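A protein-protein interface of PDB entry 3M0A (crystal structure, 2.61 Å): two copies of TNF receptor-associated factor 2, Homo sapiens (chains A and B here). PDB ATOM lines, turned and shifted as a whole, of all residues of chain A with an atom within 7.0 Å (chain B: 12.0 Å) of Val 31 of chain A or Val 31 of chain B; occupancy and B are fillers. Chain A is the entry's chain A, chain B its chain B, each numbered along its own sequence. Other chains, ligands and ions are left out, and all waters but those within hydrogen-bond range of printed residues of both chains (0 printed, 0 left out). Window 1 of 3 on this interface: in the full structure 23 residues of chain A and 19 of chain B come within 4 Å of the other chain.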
ATOM      1  N   ARG A  26      28.869  -4.485   5.788  1.00  0.00           N
ATOM      2  CA  ARG A  26      29.740  -4.116   6.885  1.00  0.00           C
ATOM      3  C   ARG A  26      29.165  -2.868   7.625  1.00  0.00           C
ATOM      4  O   ARG A  26      29.418  -2.645   8.810  1.00  0.00           O
ATOM      5  CB  ARG A  26      31.152  -3.864   6.318  1.00  0.00           C
ATOM      6  CG  ARG A  26      32.150  -3.114   7.211  1.00  0.00           C
ATOM      7  CD  ARG A  26      32.655  -3.961   8.365  1.00  0.00           C
ATOM      8  NE  ARG A  26      33.015  -3.110   9.479  1.00  0.00           N
ATOM      9  CZ  ARG A  26      32.910  -3.454  10.765  1.00  0.00           C
ATOM     10  NH1 ARG A  26      32.468  -4.674  11.153  1.00  0.00           N
ATOM     11  NH2 ARG A  26      33.246  -2.563  11.682  1.00  0.00           N
ATOM     12  N   GLU A  27      28.401  -2.055   6.901  1.00  0.00           N
ATOM     13  CA  GLU A  27      27.667  -0.924   7.468  1.00  0.00           C
ATOM     14  C   GLU A  27      26.500  -1.492   8.219  1.00  0.00           C
ATOM     15  O   GLU A  27      26.113  -0.939   9.228  1.00  0.00           O
ATOM     16  CB  GLU A  27      27.127   0.006   6.372  1.00  0.00           C
ATOM     17  CG  GLU A  27      28.002   1.174   5.999  1.00  0.00           C
ATOM     18  CD  GLU A  27      28.389   1.936   7.239  1.00  0.00           C
ATOM     19  OE1 GLU A  27      27.531   2.685   7.787  1.00  0.00           O
ATOM     20  OE2 GLU A  27      29.550   1.749   7.686  1.00  0.00           O
ATOM     21  N   VAL A  28      25.953  -2.602   7.734  1.00  0.00           N
ATOM     22  CA  VAL A  28      24.836  -3.243   8.392  1.00  0.00           C
ATOM     23  C   VAL A  28      25.269  -3.778   9.769  1.00  0.00           C
ATOM     24  O   VAL A  28      24.509  -3.661  10.740  1.00  0.00           O
ATOM     25  CB  VAL A  28      24.170  -4.330   7.498  1.00  0.00           C
ATOM     26  CG1 VAL A  28      23.102  -5.112   8.220  1.00  0.00           C
ATOM     27  CG2 VAL A  28      23.538  -3.698   6.289  1.00  0.00           C
ATOM     28  N   GLU A  29      26.498  -4.321   9.874  1.00  0.00           N
ATOM     29  CA  GLU A  29      26.985  -4.873  11.174  1.00  0.00           C
ATOM     30  C   GLU A  29      27.249  -3.768  12.123  1.00  0.00           C
ATOM     31  O   GLU A  29      26.974  -3.885  13.308  1.00  0.00           O
ATOM     32  CB  GLU A  29      28.246  -5.728  11.028  1.00  0.00           C
ATOM     33  CG  GLU A  29      27.965  -7.019  10.292  1.00  0.00           C
ATOM     34  CD  GLU A  29      29.142  -7.584   9.528  1.00  0.00           C
ATOM     35  OE1 GLU A  29      29.458  -7.106   8.419  1.00  0.00           O
ATOM     36  OE2 GLU A  29      29.741  -8.541  10.042  1.00  0.00           O
ATOM     37  N   ARG A  30      27.805  -2.680  11.611  1.00  0.00           N
ATOM     38  CA  ARG A  30      28.048  -1.567  12.480  1.00  0.00           C
ATOM     39  C   ARG A  30      26.731  -1.107  13.043  1.00  0.00           C
ATOM     40  O   ARG A  30      26.592  -0.971  14.237  1.00  0.00           O
ATOM     41  CB  ARG A  30      28.719  -0.423  11.758  1.00  0.00           C
ATOM     42  CG  ARG A  30      28.932   0.751  12.659  1.00  0.00           C
ATOM     43  CD  ARG A  30      29.867   1.772  12.100  1.00  0.00           C
ATOM     44  NE  ARG A  30      29.295   2.447  10.926  1.00  0.00           N
ATOM     45  CZ  ARG A  30      28.314   3.357  10.971  1.00  0.00           C
ATOM     46  NH1 ARG A  30      27.772   3.691  12.164  1.00  0.00           N
ATOM     47  NH2 ARG A  30      27.881   3.927   9.827  1.00  0.00           N
ATOM     48  N   VAL A  31      25.752  -0.876  12.192  1.00  0.00           N
ATOM     49  CA  VAL A  31      24.483  -0.399  12.680  1.00  0.00           C
ATOM     50  C   VAL A  31      23.817  -1.393  13.634  1.00  0.00           C
ATOM     51  O   VAL A  31      23.497  -1.017  14.774  1.00  0.00           O
ATOM     52  CB  VAL A  31      23.548  -0.050  11.559  1.00  0.00           C
ATOM     53  CG1 VAL A  31      22.165   0.142  12.096  1.00  0.00           C
ATOM     54  CG2 VAL A  31      24.028   1.219  10.856  1.00  0.00           C
ATOM     55  N   ALA A  32      23.632  -2.645  13.219  1.00  0.00           N
ATOM     56  CA  ALA A  32      23.061  -3.663  14.115  1.00  0.00           C
ATOM     57  C   ALA A  32      23.712  -3.727  15.510  1.00  0.00           C
ATOM     58  O   ALA A  32      23.052  -4.108  16.505  1.00  0.00           O
ATOM     59  CB  ALA A  32      23.125  -5.003  13.477  1.00  0.00           C
ATOM     60  N   MET A  33      24.998  -3.360  15.570  1.00  0.00           N
ATOM     61  CA  MET A  33      25.762  -3.370  16.810  1.00  0.00           C
ATOM     62  C   MET A  33      25.341  -2.199  17.699  1.00  0.00           C
ATOM     63  O   MET A  33      25.322  -2.351  18.934  1.00  0.00           O
ATOM     64  CB  MET A  33      27.288  -3.387  16.566  1.00  0.00           C
ATOM     65  N   THR A  34      24.990  -1.053  17.088  1.00  0.00           N
ATOM     66  CA  THR A  34      24.439   0.071  17.852  1.00  0.00           C
ATOM     67  C   THR A  34      22.928  -0.126  18.216  1.00  0.00           C
ATOM     68  O   THR A  34      22.464   0.393  19.228  1.00  0.00           O
ATOM     69  CB  THR A  34      24.715   1.453  17.200  1.00  0.00           C
ATOM     70  OG1 THR A  34      23.865   1.610  16.083  1.00  0.00           O
ATOM     71  CG2 THR A  34      26.187   1.639  16.756  1.00  0.00           C
ATOM     72  N   ALA A  35      22.183  -0.913  17.424  1.00  0.00           N
ATOM     73  CA  ALA A  35      20.764  -1.292  17.714  1.00  0.00           C
ATOM     74  C   ALA A  35      20.580  -2.145  18.961  1.00  0.00           C
ATOM     75  O   ALA A  35      19.843  -1.759  19.865  1.00  0.00           O
ATOM     76  CB  ALA A  35      20.125  -1.984  16.518  1.00  0.00           C
ATOM     77  N   GLU A  36      21.226  -3.309  18.997  1.00  0.00           N
ATOM     78  CA  GLU A  36      21.294  -4.124  20.209  1.00  0.00           C
ATOM     79  C   GLU A  36      21.834  -3.345  21.461  1.00  0.00           C
ATOM     80  O   GLU A  36      21.524  -3.715  22.607  1.00  0.00           O
ATOM     81  CB  GLU A  36      22.070  -5.437  19.960  1.00  0.00           C
ATOM     82  N   ALA A  37      22.602  -2.268  21.255  1.00  0.00           N
ATOM     83  CA  ALA A  37      23.099  -1.481  22.383  1.00  0.00           C
ATOM     84  C   ALA A  37      21.978  -0.638  23.000  1.00  0.00           C
ATOM     85  O   ALA A  37      21.933  -0.417  24.199  1.00  0.00           O
ATOM     86  CB  ALA A  37      24.223  -0.609  21.970  1.00  0.00           C
ATOM     87  N   CYS B  22      19.062 -10.380  -2.291  1.00  0.00           N
ATOM     88  CA  CYS B  22      17.961 -10.714  -1.343  1.00  0.00           C
ATOM     89  C   CYS B  22      18.333 -10.682   0.134  1.00  0.00           C
ATOM     90  O   CYS B  22      17.612 -10.061   0.935  1.00  0.00           O
ATOM     91  CB  CYS B  22      17.338 -12.077  -1.608  1.00  0.00           C
ATOM     92  SG  CYS B  22      16.382 -12.052  -3.097  1.00  0.00           S
ATOM     93  N   VAL B  23      19.393 -11.410   0.508  1.00  0.00           N
ATOM     94  CA  VAL B  23      19.911 -11.420   1.860  1.00  0.00           C
ATOM     95  C   VAL B  23      20.101  -9.971   2.372  1.00  0.00           C
ATOM     96  O   VAL B  23      19.461  -9.553   3.361  1.00  0.00           O
ATOM     97  CB  VAL B  23      21.216 -12.240   1.861  1.00  0.00           C
ATOM     98  CG1 VAL B  23      22.028 -12.106   3.209  1.00  0.00           C
ATOM     99  CG2 VAL B  23      20.882 -13.663   1.542  1.00  0.00           C
ATOM    100  N   LEU B  24      20.941  -9.180   1.687  1.00  0.00           N
ATOM    101  CA  LEU B  24      21.223  -7.812   2.143  1.00  0.00           C
ATOM    102  C   LEU B  24      19.933  -7.030   2.420  1.00  0.00           C
ATOM    103  O   LEU B  24      19.838  -6.193   3.367  1.00  0.00           O
ATOM    104  CB  LEU B  24      21.916  -7.108   1.036  1.00  0.00           C
ATOM    105  CG  LEU B  24      23.152  -6.380   1.474  1.00  0.00           C
ATOM    106  CD1 LEU B  24      23.511  -5.473   0.295  1.00  0.00           C
ATOM    107  CD2 LEU B  24      22.932  -5.591   2.684  1.00  0.00           C
ATOM    108  N   ASN B  25      18.951  -7.274   1.541  1.00  0.00           N
ATOM    109  CA  ASN B  25      17.682  -6.566   1.566  1.00  0.00           C
ATOM    110  C   ASN B  25      17.059  -6.833   2.888  1.00  0.00           C
ATOM    111  O   ASN B  25      16.851  -5.862   3.651  1.00  0.00           O
ATOM    112  CB  ASN B  25      16.757  -7.016   0.420  1.00  0.00           C
ATOM    113  CG  ASN B  25      15.370  -6.424   0.505  1.00  0.00           C
ATOM    114  OD1 ASN B  25      15.187  -5.251   0.771  1.00  0.00           O
ATOM    115  ND2 ASN B  25      14.392  -7.247   0.272  1.00  0.00           N
ATOM    116  N   ARG B  26      16.807  -8.131   3.167  1.00  0.00           N
ATOM    117  CA  ARG B  26      16.278  -8.614   4.481  1.00  0.00           C
ATOM    118  C   ARG B  26      17.049  -8.034   5.696  1.00  0.00           C
ATOM    119  O   ARG B  26      16.472  -7.458   6.641  1.00  0.00           O
ATOM    120  CB  ARG B  26      16.255 -10.172   4.554  1.00  0.00           C
ATOM    121  CG  ARG B  26      15.483 -10.909   3.374  1.00  0.00           C
ATOM    122  CD  ARG B  26      15.207 -12.473   3.561  1.00  0.00           C
ATOM    123  NE  ARG B  26      14.824 -13.119   2.276  1.00  0.00           N
ATOM    124  CZ  ARG B  26      15.592 -13.981   1.592  1.00  0.00           C
ATOM    125  NH1 ARG B  26      16.775 -14.349   2.082  1.00  0.00           N
ATOM    126  NH2 ARG B  26      15.189 -14.491   0.418  1.00  0.00           N
ATOM    127  N   GLU B  27      18.356  -8.149   5.645  1.00  0.00           N
ATOM    128  CA  GLU B  27      19.146  -7.775   6.756  1.00  0.00           C
ATOM    129  C   GLU B  27      19.032  -6.294   6.984  1.00  0.00           C
ATOM    130  O   GLU B  27      18.913  -5.820   8.142  1.00  0.00           O
ATOM    131  CB  GLU B  27      20.570  -8.167   6.463  1.00  0.00           C
ATOM    132  CG  GLU B  27      20.759  -9.694   6.482  1.00  0.00           C
ATOM    133  CD  GLU B  27      22.192 -10.113   6.157  1.00  0.00           C
ATOM    134  OE1 GLU B  27      22.889  -9.315   5.427  1.00  0.00           O
ATOM    135  OE2 GLU B  27      22.600 -11.237   6.617  1.00  0.00           O
ATOM    136  N   VAL B  28      19.038  -5.548   5.897  1.00  0.00           N
ATOM    137  CA  VAL B  28      18.752  -4.136   6.037  1.00  0.00           C
ATOM    138  C   VAL B  28      17.336  -3.949   6.552  1.00  0.00           C
ATOM    139  O   VAL B  28      17.136  -3.093   7.418  1.00  0.00           O
ATOM    140  CB  VAL B  28      18.946  -3.337   4.750  1.00  0.00           C
ATOM    141  CG1 VAL B  28      18.644  -1.862   5.020  1.00  0.00           C
ATOM    142  CG2 VAL B  28      20.372  -3.552   4.188  1.00  0.00           C
ATOM    143  N   GLU B  29      16.350  -4.742   6.109  1.00  0.00           N
ATOM    144  CA  GLU B  29      14.986  -4.501   6.620  1.00  0.00           C
ATOM    145  C   GLU B  29      14.951  -4.853   8.079  1.00  0.00           C
ATOM    146  O   GLU B  29      14.395  -4.077   8.880  1.00  0.00           O
ATOM    147  CB  GLU B  29      13.933  -5.341   5.931  1.00  0.00           C
ATOM    148  CG  GLU B  29      12.599  -4.672   5.911  1.00  0.00           C
ATOM    149  CD  GLU B  29      11.440  -5.579   5.421  1.00  0.00           C
ATOM    150  OE1 GLU B  29      11.631  -6.547   4.587  1.00  0.00           O
ATOM    151  OE2 GLU B  29      10.294  -5.307   5.892  1.00  0.00           O
ATOM    152  N   ARG B  30      15.537  -6.012   8.440  1.00  0.00           N
ATOM    153  CA  ARG B  30      15.584  -6.454   9.843  1.00  0.00           C
ATOM    154  C   ARG B  30      16.154  -5.330  10.654  1.00  0.00           C
ATOM    155  O   ARG B  30      15.596  -4.899  11.658  1.00  0.00           O
ATOM    156  CB  ARG B  30      16.470  -7.714  10.031  1.00  0.00           C
ATOM    157  N   VAL B  31      17.274  -4.798  10.227  1.00  0.00           N
ATOM    158  CA  VAL B  31      17.829  -3.801  11.105  1.00  0.00           C
ATOM    159  C   VAL B  31      16.938  -2.575  11.213  1.00  0.00           C
ATOM    160  O   VAL B  31      16.913  -1.897  12.231  1.00  0.00           O
ATOM    161  CB  VAL B  31      19.238  -3.456  10.686  1.00  0.00           C
ATOM    162  CG1 VAL B  31      19.859  -2.665  11.781  1.00  0.00           C
ATOM    163  CG2 VAL B  31      20.039  -4.766  10.523  1.00  0.00           C
ATOM    164  N   ALA B  32      16.183  -2.257  10.183  1.00  0.00           N
ATOM    165  CA  ALA B  32      15.485  -0.985  10.246  1.00  0.00           C
ATOM    166  C   ALA B  32      14.296  -1.153  11.127  1.00  0.00           C
ATOM    167  O   ALA B  32      13.776  -0.193  11.662  1.00  0.00           O
ATOM    168  CB  ALA B  32      15.067  -0.517   8.880  1.00  0.00           C
ATOM    169  N   MET B  33      13.846  -2.380  11.302  1.00  0.00           N
ATOM    170  CA  MET B  33      12.736  -2.604  12.189  1.00  0.00           C
ATOM    171  C   MET B  33      13.149  -2.616  13.626  1.00  0.00           C
ATOM    172  O   MET B  33      12.435  -2.069  14.462  1.00  0.00           O
ATOM    173  CB  MET B  33      12.040  -3.882  11.842  1.00  0.00           C
ATOM    174  CG  MET B  33      11.103  -3.632  10.720  1.00  0.00           C
ATOM    175  SD  MET B  33      10.147  -5.126  10.395  1.00  0.00           S
ATOM    176  CE  MET B  33       8.644  -4.717  11.361  1.00  0.00           C
ATOM    177  N   THR B  34      14.251  -3.295  13.909  1.00  0.00           N
ATOM    178  CA  THR B  34      14.913  -3.241  15.180  1.00  0.00           C
ATOM    179  C   THR B  34      15.129  -1.828  15.624  1.00  0.00           C
ATOM    180  O   THR B  34      14.818  -1.511  16.760  1.00  0.00           O
ATOM    181  CB  THR B  34      16.258  -3.798  15.037  1.00  0.00           C
ATOM    182  OG1 THR B  34      16.123  -5.186  14.809  1.00  0.00           O
ATOM    183  CG2 THR B  34      17.012  -3.624  16.249  1.00  0.00           C
ATOM    184  N   ALA B  35      15.646  -0.970  14.746  1.00  0.00           N
ATOM    185  CA  ALA B  35      15.926   0.411  15.127  1.00  0.00           C
ATOM    186  C   ALA B  35      14.683   1.264  15.389  1.00  0.00           C
ATOM    187  O   ALA B  35      14.736   2.239  16.119  1.00  0.00           O
ATOM    188  CB  ALA B  35      16.760   1.066  14.069  1.00  0.00           C
ATOM    189  N   GLU B  36      13.572   0.937  14.749  1.00  0.00           N
ATOM    190  CA  GLU B  36      12.353   1.697  14.965  1.00  0.00           C
ATOM    191  C   GLU B  36      11.538   1.162  16.153  1.00  0.00           C
ATOM    192  O   GLU B  36      10.828   1.932  16.801  1.00  0.00           O
ATOM    193  CB  GLU B  36      11.521   1.798  13.680  1.00  0.00           C
ATOM    194  CG  GLU B  36      10.141   2.523  13.816  1.00  0.00           C
ATOM    195  CD  GLU B  36      10.184   4.036  14.289  1.00  0.00           C
ATOM    196  OE1 GLU B  36       9.084   4.662  14.338  1.00  0.00           O
ATOM    197  OE2 GLU B  36      11.276   4.604  14.610  1.00  0.00           O
ATOM    198  N   ALA B  37      11.634  -0.139  16.440  1.00  0.00           N
ATOM    199  CA  ALA B  37      11.162  -0.669  17.721  1.00  0.00           C
ATOM    200  C   ALA B  37      11.976  -0.013  18.824  1.00  0.00           C
ATOM    201  O   ALA B  37      11.407   0.597  19.713  1.00  0.00           O
ATOM    202  CB  ALA B  37      11.280  -2.209  17.800  1.00  0.00           C
ATOM    203  N   CYS B  38      13.300  -0.137  18.735  1.00  0.00           N
ATOM    204  CA  CYS B  38      14.272   0.382  19.729  1.00  0.00           C
ATOM    205  C   CYS B  38      14.113   1.854  20.088  1.00  0.00           C
ATOM    206  O   CYS B  38      14.561   2.291  21.135  1.00  0.00           O
ATOM    207  CB  CYS B  38      15.701   0.181  19.179  1.00  0.00           C
ATOM    208  SG  CYS B  38      17.194   0.258  20.317  1.00  0.00           S
ATOM    209  N   SER B  39      13.495   2.614  19.190  1.00  0.00           N
ATOM    210  CA  SER B  39      13.365   4.076  19.308  1.00  0.00           C
ATOM    211  C   SER B  39      11.947   4.403  19.731  1.00  0.00           C
ATOM    212  O   SER B  39      11.539   5.551  19.764  1.00  0.00           O
ATOM    213  CB  SER B  39      13.674   4.769  17.961  1.00  0.00           C
ATOM    214  OG  SER B  39      14.548   5.876  18.112  1.00  0.00           O
ATOM    215  N   ARG B  40      11.180   3.376  20.030  1.00  0.00           N
ATOM    216  CA  ARG B  40       9.881   3.560  20.636  1.00  0.00           C
ATOM    217  C   ARG B  40       9.932   2.939  22.047  1.00  0.00           C
ATOM    218  O   ARG B  40       8.984   3.014  22.806  1.00  0.00           O
ATOM    219  CB  ARG B  40       8.829   2.902  19.756  1.00  0.00           C
ATOM    220  CG  ARG B  40       7.528   3.647  19.665  1.00  0.00           C
ATOM    221  CD  ARG B  40       6.445   2.752  19.070  1.00  0.00           C
ATOM    222  NE  ARG B  40       6.743   2.302  17.703  1.00  0.00           N
ATOM    223  CZ  ARG B  40       6.275   2.869  16.587  1.00  0.00           C
ATOM    224  NH1 ARG B  40       5.474   3.942  16.637  1.00  0.00           N
ATOM    225  NH2 ARG B  40       6.615   2.351  15.407  1.00  0.00           N
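The side-chain sulfur of Cys 38 of chain B is in hydrogen-bond range of the backbone carbonyl oxygen of Ala 35 of chain A, at 3.4 Å.
O of Arg 30 of chain B is in hydrogen-bond range of OG1 of Thr 34 of chain B, 3.2 Å away.
O of Val 31 of chain A is in hydrogen-bond range of OG1 of Thr 34 of chain A.
Val 28 of chain A touches Val 28 of chain B.
Val 31 of chain B touches Val 28 of chain A.
Val 31 of chain A touches Val 31 of chain B (CG1 to CG1, 3.6 Å).
CB of Ala 35 of chain A touches CG2 of Thr 34 of chain B (3.5 Å).
Printed residues of chain B within 4 Å of Val 31 of chain A: Val 31 (3.6 Å).
No residue of chain B comes within 4 Å of Arg 30 of chain A.
No residue of chain B comes within 4 Å of Thr 34 of chain A.
Of the printed residues of chain A, Thr 34 of chain B touches Ala 35 (3.5 Å).
Of the printed residues of chain A, Val 28 of chain B touches Val 28 (3.8 Å).
Printed residues of chain A within 4 Å of Cys 38 of chain B: Ala 35 (3.4 Å).
Ala 32 of chain B touches none of the printed residues of chain A.
Ala 37 of chain A touches none of the printed residues of chain B.
Of the 12 printed residues of chain A, 3 touch a printed residue of chain B.
Hydrophobic or aromatic side chains of chain A within 4 Å of the printed part of chain B: Val 28, Val 31 and Ala 35.
Of the 19 printed residues of chain B, 4 touch a printed residue of chain A.
Among the printed residues, 5 pairs touch across the chains.
Val 28 of chain B touches its own counterpart, Val 28 of chain A.
Val 28 of chain A touches Val 31 of chain B, but with the chains exchanged Val 31 of chain A does not touch Val 28 of chain B (7.6 Å).
Val 31 of chain A touches its own counterpart, Val 31 of chain B.
Ala 35 of chain A touches Thr 34 of chain B, but with the chains exchanged Thr 34 of chain A does not touch Ala 35 of chain B (7.4 Å).
12 positions are printed for both chains.
Of the 5 pairs that touch across the chains among the printed residues, 2 have their exchanged pair printed and touching as well.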
